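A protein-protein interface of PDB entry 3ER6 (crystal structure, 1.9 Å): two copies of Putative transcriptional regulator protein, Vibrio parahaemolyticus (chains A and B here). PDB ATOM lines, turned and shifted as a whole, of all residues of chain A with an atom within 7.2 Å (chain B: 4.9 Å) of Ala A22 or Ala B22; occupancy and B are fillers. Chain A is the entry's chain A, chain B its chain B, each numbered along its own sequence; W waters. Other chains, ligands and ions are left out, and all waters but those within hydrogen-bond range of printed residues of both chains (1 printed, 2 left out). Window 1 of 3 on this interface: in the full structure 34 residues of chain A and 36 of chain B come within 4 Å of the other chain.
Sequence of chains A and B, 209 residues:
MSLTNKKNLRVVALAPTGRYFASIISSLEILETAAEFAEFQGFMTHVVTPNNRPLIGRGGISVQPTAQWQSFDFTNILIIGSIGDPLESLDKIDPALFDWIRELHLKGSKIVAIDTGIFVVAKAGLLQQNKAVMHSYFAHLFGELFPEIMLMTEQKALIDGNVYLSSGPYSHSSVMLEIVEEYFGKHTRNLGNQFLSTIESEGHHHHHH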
ATOM      1  N   THR A  17       9.265 -10.153   4.070  1.00  0.00           N
ATOM      2  CA  THR A  17       7.977  -9.836   4.710  1.00  0.00           C
ATOM      3  C   THR A  17       7.479  -8.434   4.394  1.00  0.00           C
ATOM      4  O   THR A  17       8.257  -7.462   4.450  1.00  0.00           O
ATOM      5  CB  THR A  17       8.033 -10.038   6.276  1.00  0.00           C
ATOM      6  OG1 THR A  17       6.791  -9.596   6.870  1.00  0.00           O
ATOM      7  CG2 THR A  17       9.114  -9.262   6.893  1.00  0.00           C
ATOM      8  N   GLY A  18       6.172  -8.298   4.127  1.00  0.00           N
ATOM      9  CA  GLY A  18       5.597  -6.989   3.906  1.00  0.00           C
ATOM     10  C   GLY A  18       5.481  -6.166   5.192  1.00  0.00           C
ATOM     11  O   GLY A  18       5.207  -4.987   5.153  1.00  0.00           O
ATOM     12  N   ARG A  19       5.735  -6.762   6.335  1.00  0.00           N
ATOM     13  CA  ARG A  19       5.784  -5.988   7.573  1.00  0.00           C
ATOM     14  C   ARG A  19       6.963  -5.012   7.601  1.00  0.00           C
ATOM     15  O   ARG A  19       6.870  -3.930   8.218  1.00  0.00           O
ATOM     16  CB  ARG A  19       5.858  -6.940   8.781  1.00  0.00           C
ATOM     17  CG  ARG A  19       4.649  -7.950   8.937  1.00  0.00           C
ATOM     18  CD  ARG A  19       3.285  -7.241   9.217  1.00  0.00           C
ATOM     19  NE  ARG A  19       2.678  -6.781   7.960  1.00  0.00           N
ATOM     20  CZ  ARG A  19       1.667  -5.912   7.893  1.00  0.00           C
ATOM     21  NH1 ARG A  19       1.204  -5.526   6.731  1.00  0.00           N
ATOM     22  NH2 ARG A  19       1.134  -5.407   9.000  1.00  0.00           N
ATOM     23  N   TYR A  20       8.048  -5.361   6.891  1.00  0.00           N
ATOM     24  CA  TYR A  20       9.270  -4.590   6.935  1.00  0.00           C
ATOM     25  C   TYR A  20       9.959  -4.739   5.605  1.00  0.00           C
ATOM     26  O   TYR A  20      10.914  -5.516   5.473  1.00  0.00           O
ATOM     27  CB  TYR A  20      10.192  -5.125   8.073  1.00  0.00           C
ATOM     28  CG  TYR A  20       9.570  -4.843   9.429  1.00  0.00           C
ATOM     29  CD1 TYR A  20       9.515  -3.534   9.927  1.00  0.00           C
ATOM     30  CD2 TYR A  20       8.998  -5.874  10.197  1.00  0.00           C
ATOM     31  CE1 TYR A  20       8.923  -3.269  11.208  1.00  0.00           C
ATOM     32  CE2 TYR A  20       8.372  -5.624  11.417  1.00  0.00           C
ATOM     33  CZ  TYR A  20       8.348  -4.355  11.931  1.00  0.00           C
ATOM     34  OH  TYR A  20       7.751  -4.141  13.165  1.00  0.00           O
ATOM     35  N   PHE A  21       9.414  -4.100   4.581  1.00  0.00           N
ATOM     36  CA  PHE A  21      10.072  -4.160   3.258  1.00  0.00           C
ATOM     37  C   PHE A  21      10.589  -2.807   2.787  1.00  0.00           C
ATOM     38  O   PHE A  21      11.312  -2.748   1.764  1.00  0.00           O
ATOM     39  CB  PHE A  21       9.175  -4.805   2.186  1.00  0.00           C
ATOM     40  CG  PHE A  21       8.102  -3.877   1.637  1.00  0.00           C
ATOM     41  CD1 PHE A  21       8.226  -3.298   0.387  1.00  0.00           C
ATOM     42  CD2 PHE A  21       6.943  -3.606   2.392  1.00  0.00           C
ATOM     43  CE1 PHE A  21       7.222  -2.431  -0.120  1.00  0.00           C
ATOM     44  CE2 PHE A  21       5.940  -2.772   1.878  1.00  0.00           C
ATOM     45  CZ  PHE A  21       6.089  -2.169   0.625  1.00  0.00           C
ATOM     46  N   ALA A  22      10.265  -1.723   3.512  1.00  0.00           N
ATOM     47  CA  ALA A  22      10.713  -0.368   3.061  1.00  0.00           C
ATOM     48  C   ALA A  22      12.192  -0.292   2.831  1.00  0.00           C
ATOM     49  O   ALA A  22      12.630   0.321   1.863  1.00  0.00           O
ATOM     50  CB  ALA A  22      10.342   0.707   4.049  1.00  0.00           C
ATOM     51  N   SER A  23      13.003  -0.894   3.709  1.00  0.00           N
ATOM     52  CA  SER A  23      14.469  -0.776   3.491  1.00  0.00           C
ATOM     53  C   SER A  23      14.989  -1.483   2.219  1.00  0.00           C
ATOM     54  O   SER A  23      16.061  -1.100   1.659  1.00  0.00           O
ATOM     55  CB  SER A  23      15.266  -1.231   4.745  1.00  0.00           C
ATOM     56  OG  SER A  23      14.973  -2.609   5.083  1.00  0.00           O
ATOM     57  N   ILE A  24      14.289  -2.518   1.773  1.00  0.00           N
ATOM     58  CA  ILE A  24      14.618  -3.117   0.473  1.00  0.00           C
ATOM     59  C   ILE A  24      14.372  -2.076  -0.618  1.00  0.00           C
ATOM     60  O   ILE A  24      15.198  -1.868  -1.500  1.00  0.00           O
ATOM     61  CB  ILE A  24      13.732  -4.366   0.221  1.00  0.00           C
ATOM     62  CG1 ILE A  24      14.330  -5.556   0.976  1.00  0.00           C
ATOM     63  CG2 ILE A  24      13.624  -4.724  -1.274  1.00  0.00           C
ATOM     64  CD1 ILE A  24      15.767  -6.002   0.363  1.00  0.00           C
ATOM     65  N   ILE A  25      13.214  -1.431  -0.561  1.00  0.00           N
ATOM     66  CA  ILE A  25      12.831  -0.435  -1.604  1.00  0.00           C
ATOM     67  C   ILE A  25      13.816   0.759  -1.533  1.00  0.00           C
ATOM     68  O   ILE A  25      14.278   1.236  -2.561  1.00  0.00           O
ATOM     69  CB  ILE A  25      11.408   0.112  -1.337  1.00  0.00           C
ATOM     70  CG1 ILE A  25      10.400  -1.029  -1.111  1.00  0.00           C
ATOM     71  CG2 ILE A  25      10.935   1.134  -2.473  1.00  0.00           C
ATOM     72  CD1 ILE A  25      10.379  -2.006  -2.312  1.00  0.00           C
ATOM     73  N   SER A  26      14.144   1.262  -0.321  1.00  0.00           N
ATOM     74  CA  SER A  26      15.059   2.416  -0.265  1.00  0.00           C
ATOM     75  C   SER A  26      16.443   2.042  -0.845  1.00  0.00           C
ATOM     76  O   SER A  26      17.071   2.870  -1.498  1.00  0.00           O
ATOM     77  CB  SER A  26      15.187   2.979   1.163  1.00  0.00           C
ATOM     78  OG  SER A  26      15.754   2.017   2.026  1.00  0.00           O
ATOM     79  N   SER A  27      16.884   0.803  -0.634  1.00  0.00           N
ATOM     80  CA  SER A  27      18.185   0.377  -1.111  1.00  0.00           C
ATOM     81  C   SER A  27      18.178   0.398  -2.627  1.00  0.00           C
ATOM     82  O   SER A  27      19.137   0.847  -3.209  1.00  0.00           O
ATOM     83  CB  SER A  27      18.591  -1.020  -0.609  1.00  0.00           C
ATOM     84  OG  SER A  27      18.616  -1.054   0.820  1.00  0.00           O
ATOM     85  N   LEU A  28      17.100  -0.083  -3.256  1.00  0.00           N
ATOM     86  CA  LEU A  28      17.020  -0.010  -4.708  1.00  0.00           C
ATOM     87  C   LEU A  28      16.917   1.420  -5.224  1.00  0.00           C
ATOM     88  O   LEU A  28      17.468   1.747  -6.291  1.00  0.00           O
ATOM     89  CB  LEU A  28      15.827  -0.839  -5.245  1.00  0.00           C
ATOM     90  CG  LEU A  28      15.912  -2.352  -4.958  1.00  0.00           C
ATOM     91  CD1 LEU A  28      14.767  -3.119  -5.621  1.00  0.00           C
ATOM     92  CD2 LEU A  28      17.316  -2.973  -5.309  1.00  0.00           C
ATOM     93  N   GLU A  29      16.158   2.259  -4.534  1.00  0.00           N
ATOM     94  CA  GLU A  29      16.092   3.657  -4.958  1.00  0.00           C
ATOM     95  C   GLU A  29      17.478   4.241  -4.931  1.00  0.00           C
ATOM     96  O   GLU A  29      17.825   5.002  -5.827  1.00  0.00           O
ATOM     97  CB  GLU A  29      15.195   4.433  -3.970  1.00  0.00           C
ATOM     98  CG  GLU A  29      13.700   4.046  -4.234  1.00  0.00           C
ATOM     99  CD  GLU A  29      12.649   4.690  -3.273  1.00  0.00           C
ATOM    100  OE1 GLU A  29      13.007   5.544  -2.477  1.00  0.00           O
ATOM    101  OE2 GLU A  29      11.475   4.282  -3.361  1.00  0.00           O
ATOM    102  N   SER A  82      14.738  -7.398   5.713  1.00  0.00           N
ATOM    103  CA  SER A  82      14.194  -7.738   7.017  1.00  0.00           C
ATOM    104  C   SER A  82      13.346  -8.999   7.032  1.00  0.00           C
ATOM    105  O   SER A  82      12.563  -9.290   6.105  1.00  0.00           O
ATOM    106  CB  SER A  82      13.341  -6.566   7.548  1.00  0.00           C
ATOM    107  OG  SER A  82      12.991  -6.823   8.887  1.00  0.00           O
ATOM    108  N   ILE A 114      20.429  -6.642   5.438  1.00  0.00           N
ATOM    109  CA  ILE A 114      20.015  -5.425   6.130  1.00  0.00           C
ATOM    110  C   ILE A 114      19.000  -5.754   7.207  1.00  0.00           C
ATOM    111  O   ILE A 114      18.142  -6.640   6.978  1.00  0.00           O
ATOM    112  CB  ILE A 114      19.459  -4.352   5.059  1.00  0.00           C
ATOM    113  CG1 ILE A 114      18.204  -4.846   4.349  1.00  0.00           C
ATOM    114  CG2 ILE A 114      20.535  -4.097   3.956  1.00  0.00           C
ATOM    115  CD1 ILE A 114      17.593  -3.779   3.382  1.00  0.00           C
ATOM    116  N   PRO A 169      17.689  -0.038  11.422  1.00  0.00           N
ATOM    117  CA  PRO A 169      16.861  -0.686  10.368  1.00  0.00           C
ATOM    118  C   PRO A 169      16.656   0.116   9.060  1.00  0.00           C
ATOM    119  O   PRO A 169      16.357  -0.522   8.018  1.00  0.00           O
ATOM    120  CB  PRO A 169      15.516  -0.940  11.090  1.00  0.00           C
ATOM    121  CG  PRO A 169      15.501   0.185  12.210  1.00  0.00           C
ATOM    122  CD  PRO A 169      16.927   0.198  12.670  1.00  0.00           C
ATOM    123  N   TYR A 170      16.768   1.450   9.084  1.00  0.00           N
ATOM    124  CA  TYR A 170      16.435   2.237   7.882  1.00  0.00           C
ATOM    125  C   TYR A 170      17.585   2.977   7.214  1.00  0.00           C
ATOM    126  O   TYR A 170      17.440   3.452   6.056  1.00  0.00           O
ATOM    127  CB  TYR A 170      15.267   3.243   8.108  1.00  0.00           C
ATOM    128  CG  TYR A 170      14.070   2.435   8.474  1.00  0.00           C
ATOM    129  CD1 TYR A 170      13.440   1.652   7.512  1.00  0.00           C
ATOM    130  CD2 TYR A 170      13.646   2.335   9.811  1.00  0.00           C
ATOM    131  CE1 TYR A 170      12.337   0.843   7.871  1.00  0.00           C
ATOM    132  CE2 TYR A 170      12.559   1.511  10.177  1.00  0.00           C
ATOM    133  CZ  TYR A 170      11.924   0.779   9.173  1.00  0.00           C
ATOM    134  OH  TYR A 170      10.879  -0.058   9.472  1.00  0.00           O
ATOM    135  N   TYR B  20      10.093   7.083  -5.880  1.00  0.00           N
ATOM    136  CA  TYR B  20      10.620   7.403  -4.550  1.00  0.00           C
ATOM    137  C   TYR B  20       9.500   7.245  -3.523  1.00  0.00           C
ATOM    138  O   TYR B  20       8.912   8.227  -3.138  1.00  0.00           O
ATOM    139  CB  TYR B  20      11.228   8.818  -4.512  1.00  0.00           C
ATOM    140  CG  TYR B  20      12.514   8.893  -5.334  1.00  0.00           C
ATOM    141  CD1 TYR B  20      13.711   8.353  -4.845  1.00  0.00           C
ATOM    142  CD2 TYR B  20      12.486   9.401  -6.628  1.00  0.00           C
ATOM    143  CE1 TYR B  20      14.897   8.388  -5.637  1.00  0.00           C
ATOM    144  CE2 TYR B  20      13.645   9.463  -7.422  1.00  0.00           C
ATOM    145  CZ  TYR B  20      14.825   8.900  -6.943  1.00  0.00           C
ATOM    146  OH  TYR B  20      15.981   8.977  -7.712  1.00  0.00           O
ATOM    147  N   PHE B  21       9.179   6.032  -3.118  1.00  0.00           N
ATOM    148  CA  PHE B  21       8.076   5.837  -2.116  1.00  0.00           C
ATOM    149  C   PHE B  21       8.521   5.095  -0.840  1.00  0.00           C
ATOM    150  O   PHE B  21       7.745   4.958   0.118  1.00  0.00           O
ATOM    151  CB  PHE B  21       6.836   5.169  -2.719  1.00  0.00           C
ATOM    152  CG  PHE B  21       6.967   3.687  -2.932  1.00  0.00           C
ATOM    153  CD1 PHE B  21       6.453   2.788  -2.032  1.00  0.00           C
ATOM    154  CD2 PHE B  21       7.617   3.194  -4.083  1.00  0.00           C
ATOM    155  CE1 PHE B  21       6.628   1.371  -2.223  1.00  0.00           C
ATOM    156  CE2 PHE B  21       7.797   1.849  -4.257  1.00  0.00           C
ATOM    157  CZ  PHE B  21       7.299   0.925  -3.329  1.00  0.00           C
ATOM    158  N   ALA B  22       9.746   4.583  -0.840  1.00  0.00           N
ATOM    159  CA  ALA B  22      10.224   3.845   0.305  1.00  0.00           C
ATOM    160  C   ALA B  22      10.043   4.618   1.605  1.00  0.00           C
ATOM    161  O   ALA B  22       9.796   4.027   2.654  1.00  0.00           O
ATOM    162  CB  ALA B  22      11.690   3.494   0.147  1.00  0.00           C
ATOM    163  N   SER B  23      10.269   5.910   1.558  1.00  0.00           N
ATOM    164  CA  SER B  23      10.249   6.696   2.810  1.00  0.00           C
ATOM    165  C   SER B  23       8.838   6.851   3.381  1.00  0.00           C
ATOM    166  O   SER B  23       8.670   7.107   4.608  1.00  0.00           O
ATOM    167  CB  SER B  23      10.908   8.060   2.625  1.00  0.00           C
ATOM    168  OG  SER B  23      10.249   8.852   1.633  1.00  0.00           O
ATOM    169  N   ILE B  24       7.824   6.760   2.512  1.00  0.00           N
ATOM    170  CA  ILE B  24       6.431   6.599   3.028  1.00  0.00           C
ATOM    171  C   ILE B  24       6.260   5.316   3.814  1.00  0.00           C
ATOM    172  O   ILE B  24       5.733   5.288   4.968  1.00  0.00           O
ATOM    173  CB  ILE B  24       5.396   6.649   1.859  1.00  0.00           C
ATOM    174  CG1 ILE B  24       5.181   8.108   1.422  1.00  0.00           C
ATOM    175  CG2 ILE B  24       4.059   5.945   2.216  1.00  0.00           C
ATOM    176  CD1 ILE B  24       4.493   9.040   2.387  1.00  0.00           C
ATOM    177  N   ILE B  25       6.726   4.234   3.215  1.00  0.00           N
ATOM    178  CA  ILE B  25       6.600   2.883   3.817  1.00  0.00           C
ATOM    179  C   ILE B  25       7.361   2.784   5.119  1.00  0.00           C
ATOM    180  O   ILE B  25       6.817   2.304   6.136  1.00  0.00           O
ATOM    181  CB  ILE B  25       7.039   1.754   2.812  1.00  0.00           C
ATOM    182  CG1 ILE B  25       6.377   1.948   1.434  1.00  0.00           C
ATOM    183  CG2 ILE B  25       6.669   0.317   3.404  1.00  0.00           C
ATOM    184  CD1 ILE B  25       4.820   2.067   1.540  1.00  0.00           C
ATOM    185  N   SER B  26       8.613   3.219   5.137  1.00  0.00           N
ATOM    186  CA  SER B  26       9.329   3.207   6.421  1.00  0.00           C
ATOM    187  C   SER B  26       8.612   4.033   7.528  1.00  0.00           C
ATOM    188  O   SER B  26       8.611   3.673   8.710  1.00  0.00           O
ATOM    189  CB  SER B  26      10.760   3.680   6.223  1.00  0.00           C
ATOM    190  OG  SER B  26      10.908   5.028   5.773  1.00  0.00           O
ATOM    191  N   GLU B  29       5.987   1.864   8.903  1.00  0.00           N
ATOM    192  CA  GLU B  29       6.530   0.750   9.679  1.00  0.00           C
ATOM    193  C   GLU B  29       6.923   1.243  11.089  1.00  0.00           C
ATOM    194  O   GLU B  29       6.619   0.553  12.105  1.00  0.00           O
ATOM    195  CB  GLU B  29       7.734   0.114   8.948  1.00  0.00           C
ATOM    196  CG  GLU B  29       7.318  -0.531   7.628  1.00  0.00           C
ATOM    197  CD  GLU B  29       8.517  -1.143   6.804  1.00  0.00           C
ATOM    198  OE1 GLU B  29       9.660  -1.023   7.267  1.00  0.00           O
ATOM    199  OE2 GLU B  29       8.244  -1.717   5.711  1.00  0.00           O
ATOM    200  N   TYR B 170      15.795   9.599   3.570  1.00  0.00           N
ATOM    201  CA  TYR B 170      15.375   8.341   4.167  1.00  0.00           C
ATOM    202  C   TYR B 170      15.354   8.252   5.692  1.00  0.00           C
ATOM    203  O   TYR B 170      14.746   7.297   6.266  1.00  0.00           O
ATOM    204  CB  TYR B 170      16.174   7.164   3.602  1.00  0.00           C
ATOM    205  CG  TYR B 170      15.980   7.050   2.110  1.00  0.00           C
ATOM    206  CD1 TYR B 170      14.753   6.621   1.576  1.00  0.00           C
ATOM    207  CD2 TYR B 170      17.017   7.410   1.228  1.00  0.00           C
ATOM    208  CE1 TYR B 170      14.582   6.528   0.204  1.00  0.00           C
ATOM    209  CE2 TYR B 170      16.842   7.364  -0.127  1.00  0.00           C
ATOM    210  CZ  TYR B 170      15.630   6.890  -0.626  1.00  0.00           C
ATOM    211  OH  TYR B 170      15.447   6.835  -1.968  1.00  0.00           O
HETATM  212  O   HOH W   1       5.403  -2.294   5.261  1.00  0.00           O
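Water W1 bridges the backbone carbonyl oxygen of Gly A18 (2.7 Å) and the side-chain carboxylate of Glu B29 (2.9 Å).
OE2 of Glu B29 lies within hydrogen-bond range of N of Phe A21 (2.9 Å).
The side-chain hydroxyl of Tyr A170 lies within hydrogen-bond range of the side-chain carboxylate of Glu B29.
The backbone NH of Ala A22 sits at hydrogen-bond distance from the side-chain carboxylate of Glu B29.
N of Phe B21 sits at hydrogen-bond distance from OE2 of Glu A29, 2.9 Å away.
OE1 of Glu A29 lies within hydrogen-bond range of OH of Tyr B170, 2.8 Å away.
The side-chain carboxylate (OE2) of Glu A29 lies within hydrogen-bond range of the backbone NH (N) of Ala B22 (3.1 Å).
The side-chain hydroxyl (OG1) of Thr A17 lies within hydrogen-bond range of the backbone NH (N) of Arg A19 (3.1 Å).
The backbone carbonyl oxygen of Ser A23 lies within hydrogen-bond range of the side-chain hydroxyl of Ser A26.
The backbone carbonyl oxygen (O) of Ser B23 sits at hydrogen-bond distance from the side-chain hydroxyl (OG) of Ser B26 (3.3 Å).
The backbone carbonyl oxygen of Ala B22 lies within hydrogen-bond range of the side-chain hydroxyl of Ser B26, at 3.5 Å.
Phe A21 touches Glu B29, and with the chains exchanged Glu A29 touches Phe B21.
Ala A22 touches Ile B25, and with the chains exchanged Ile A25 touches Ala B22.
Ala A22 touches Ser B26, and with the chains exchanged Ser A26 touches Ala B22.
Glu A29 touches Tyr B170, and with the chains exchanged Tyr A170 touches Glu B29.
Positions printed for both chains: 20, 21, 22, 23, 24, 25, 26, 29 and 170.
Of the 18 pairs that touch across the chains among the printed residues, 17 have their exchanged pair printed and touching as well.
Of the printed residues of chain B, Tyr A20 touches Glu B29.
Ala A22 touches just these residues of chain B: Ala B22, Ile B25, Ser B26 and Glu B29.
Of the printed residues of chain B, Ser A26 touches Ala B22 (3.4 Å) and Tyr B170 (3.7 Å).
Of the printed residues of chain A, Phe B21 touches Ile A25 (3.7 Å) and Glu A29 (2.9 Å).
Ala B22 touches just these residues of chain A: Ala A22, Ile A25, Ser A26 and Glu A29.
Ile B24 touches none of the printed residues of chain A.
The nearest printed residue of chain A that does not touch Tyr B20 is Ile A25 (6.4 Å).
O of Arg A19 touches CG of Glu B29, 3.5 Å away.
Glu B29 touches Tyr A20 (OE2 to CA, 3.3 Å).
CE2 of Phe A21 touches CG2 of Ile B25, at 3.5 Å.
O of Ala B22 touches CB of Ala A22 (3.6 Å).
CB of Ile B25 touches CB of Ala A22 (3.7 Å).
Ile A25 touches Ala B22.
Ser A26 touches Ala B22.
Ser A26 touches Tyr B170 (CB to CD1, 3.7 Å).
Glu A29 touches Tyr B20 (OE2 to CA, 3.4 Å).
CD1 of Tyr A170 touches CB of Ser B26 (3.6 Å).
Along chain B the printed residues that touch a printed residue of chain A span positions 20 to 170.
Hydrophobic or aromatic side chains of chain A within 4 Å of the printed part of chain B: Tyr A20, Phe A21, Ala A22, Ile A25 and Tyr A170.
Among the printed residues, 18 pairs touch across the chains.
Among the printed residues, no Asp or Glu carboxylate lies within 4 Å of a Lys or Arg side-chain nitrogen of the other chain.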
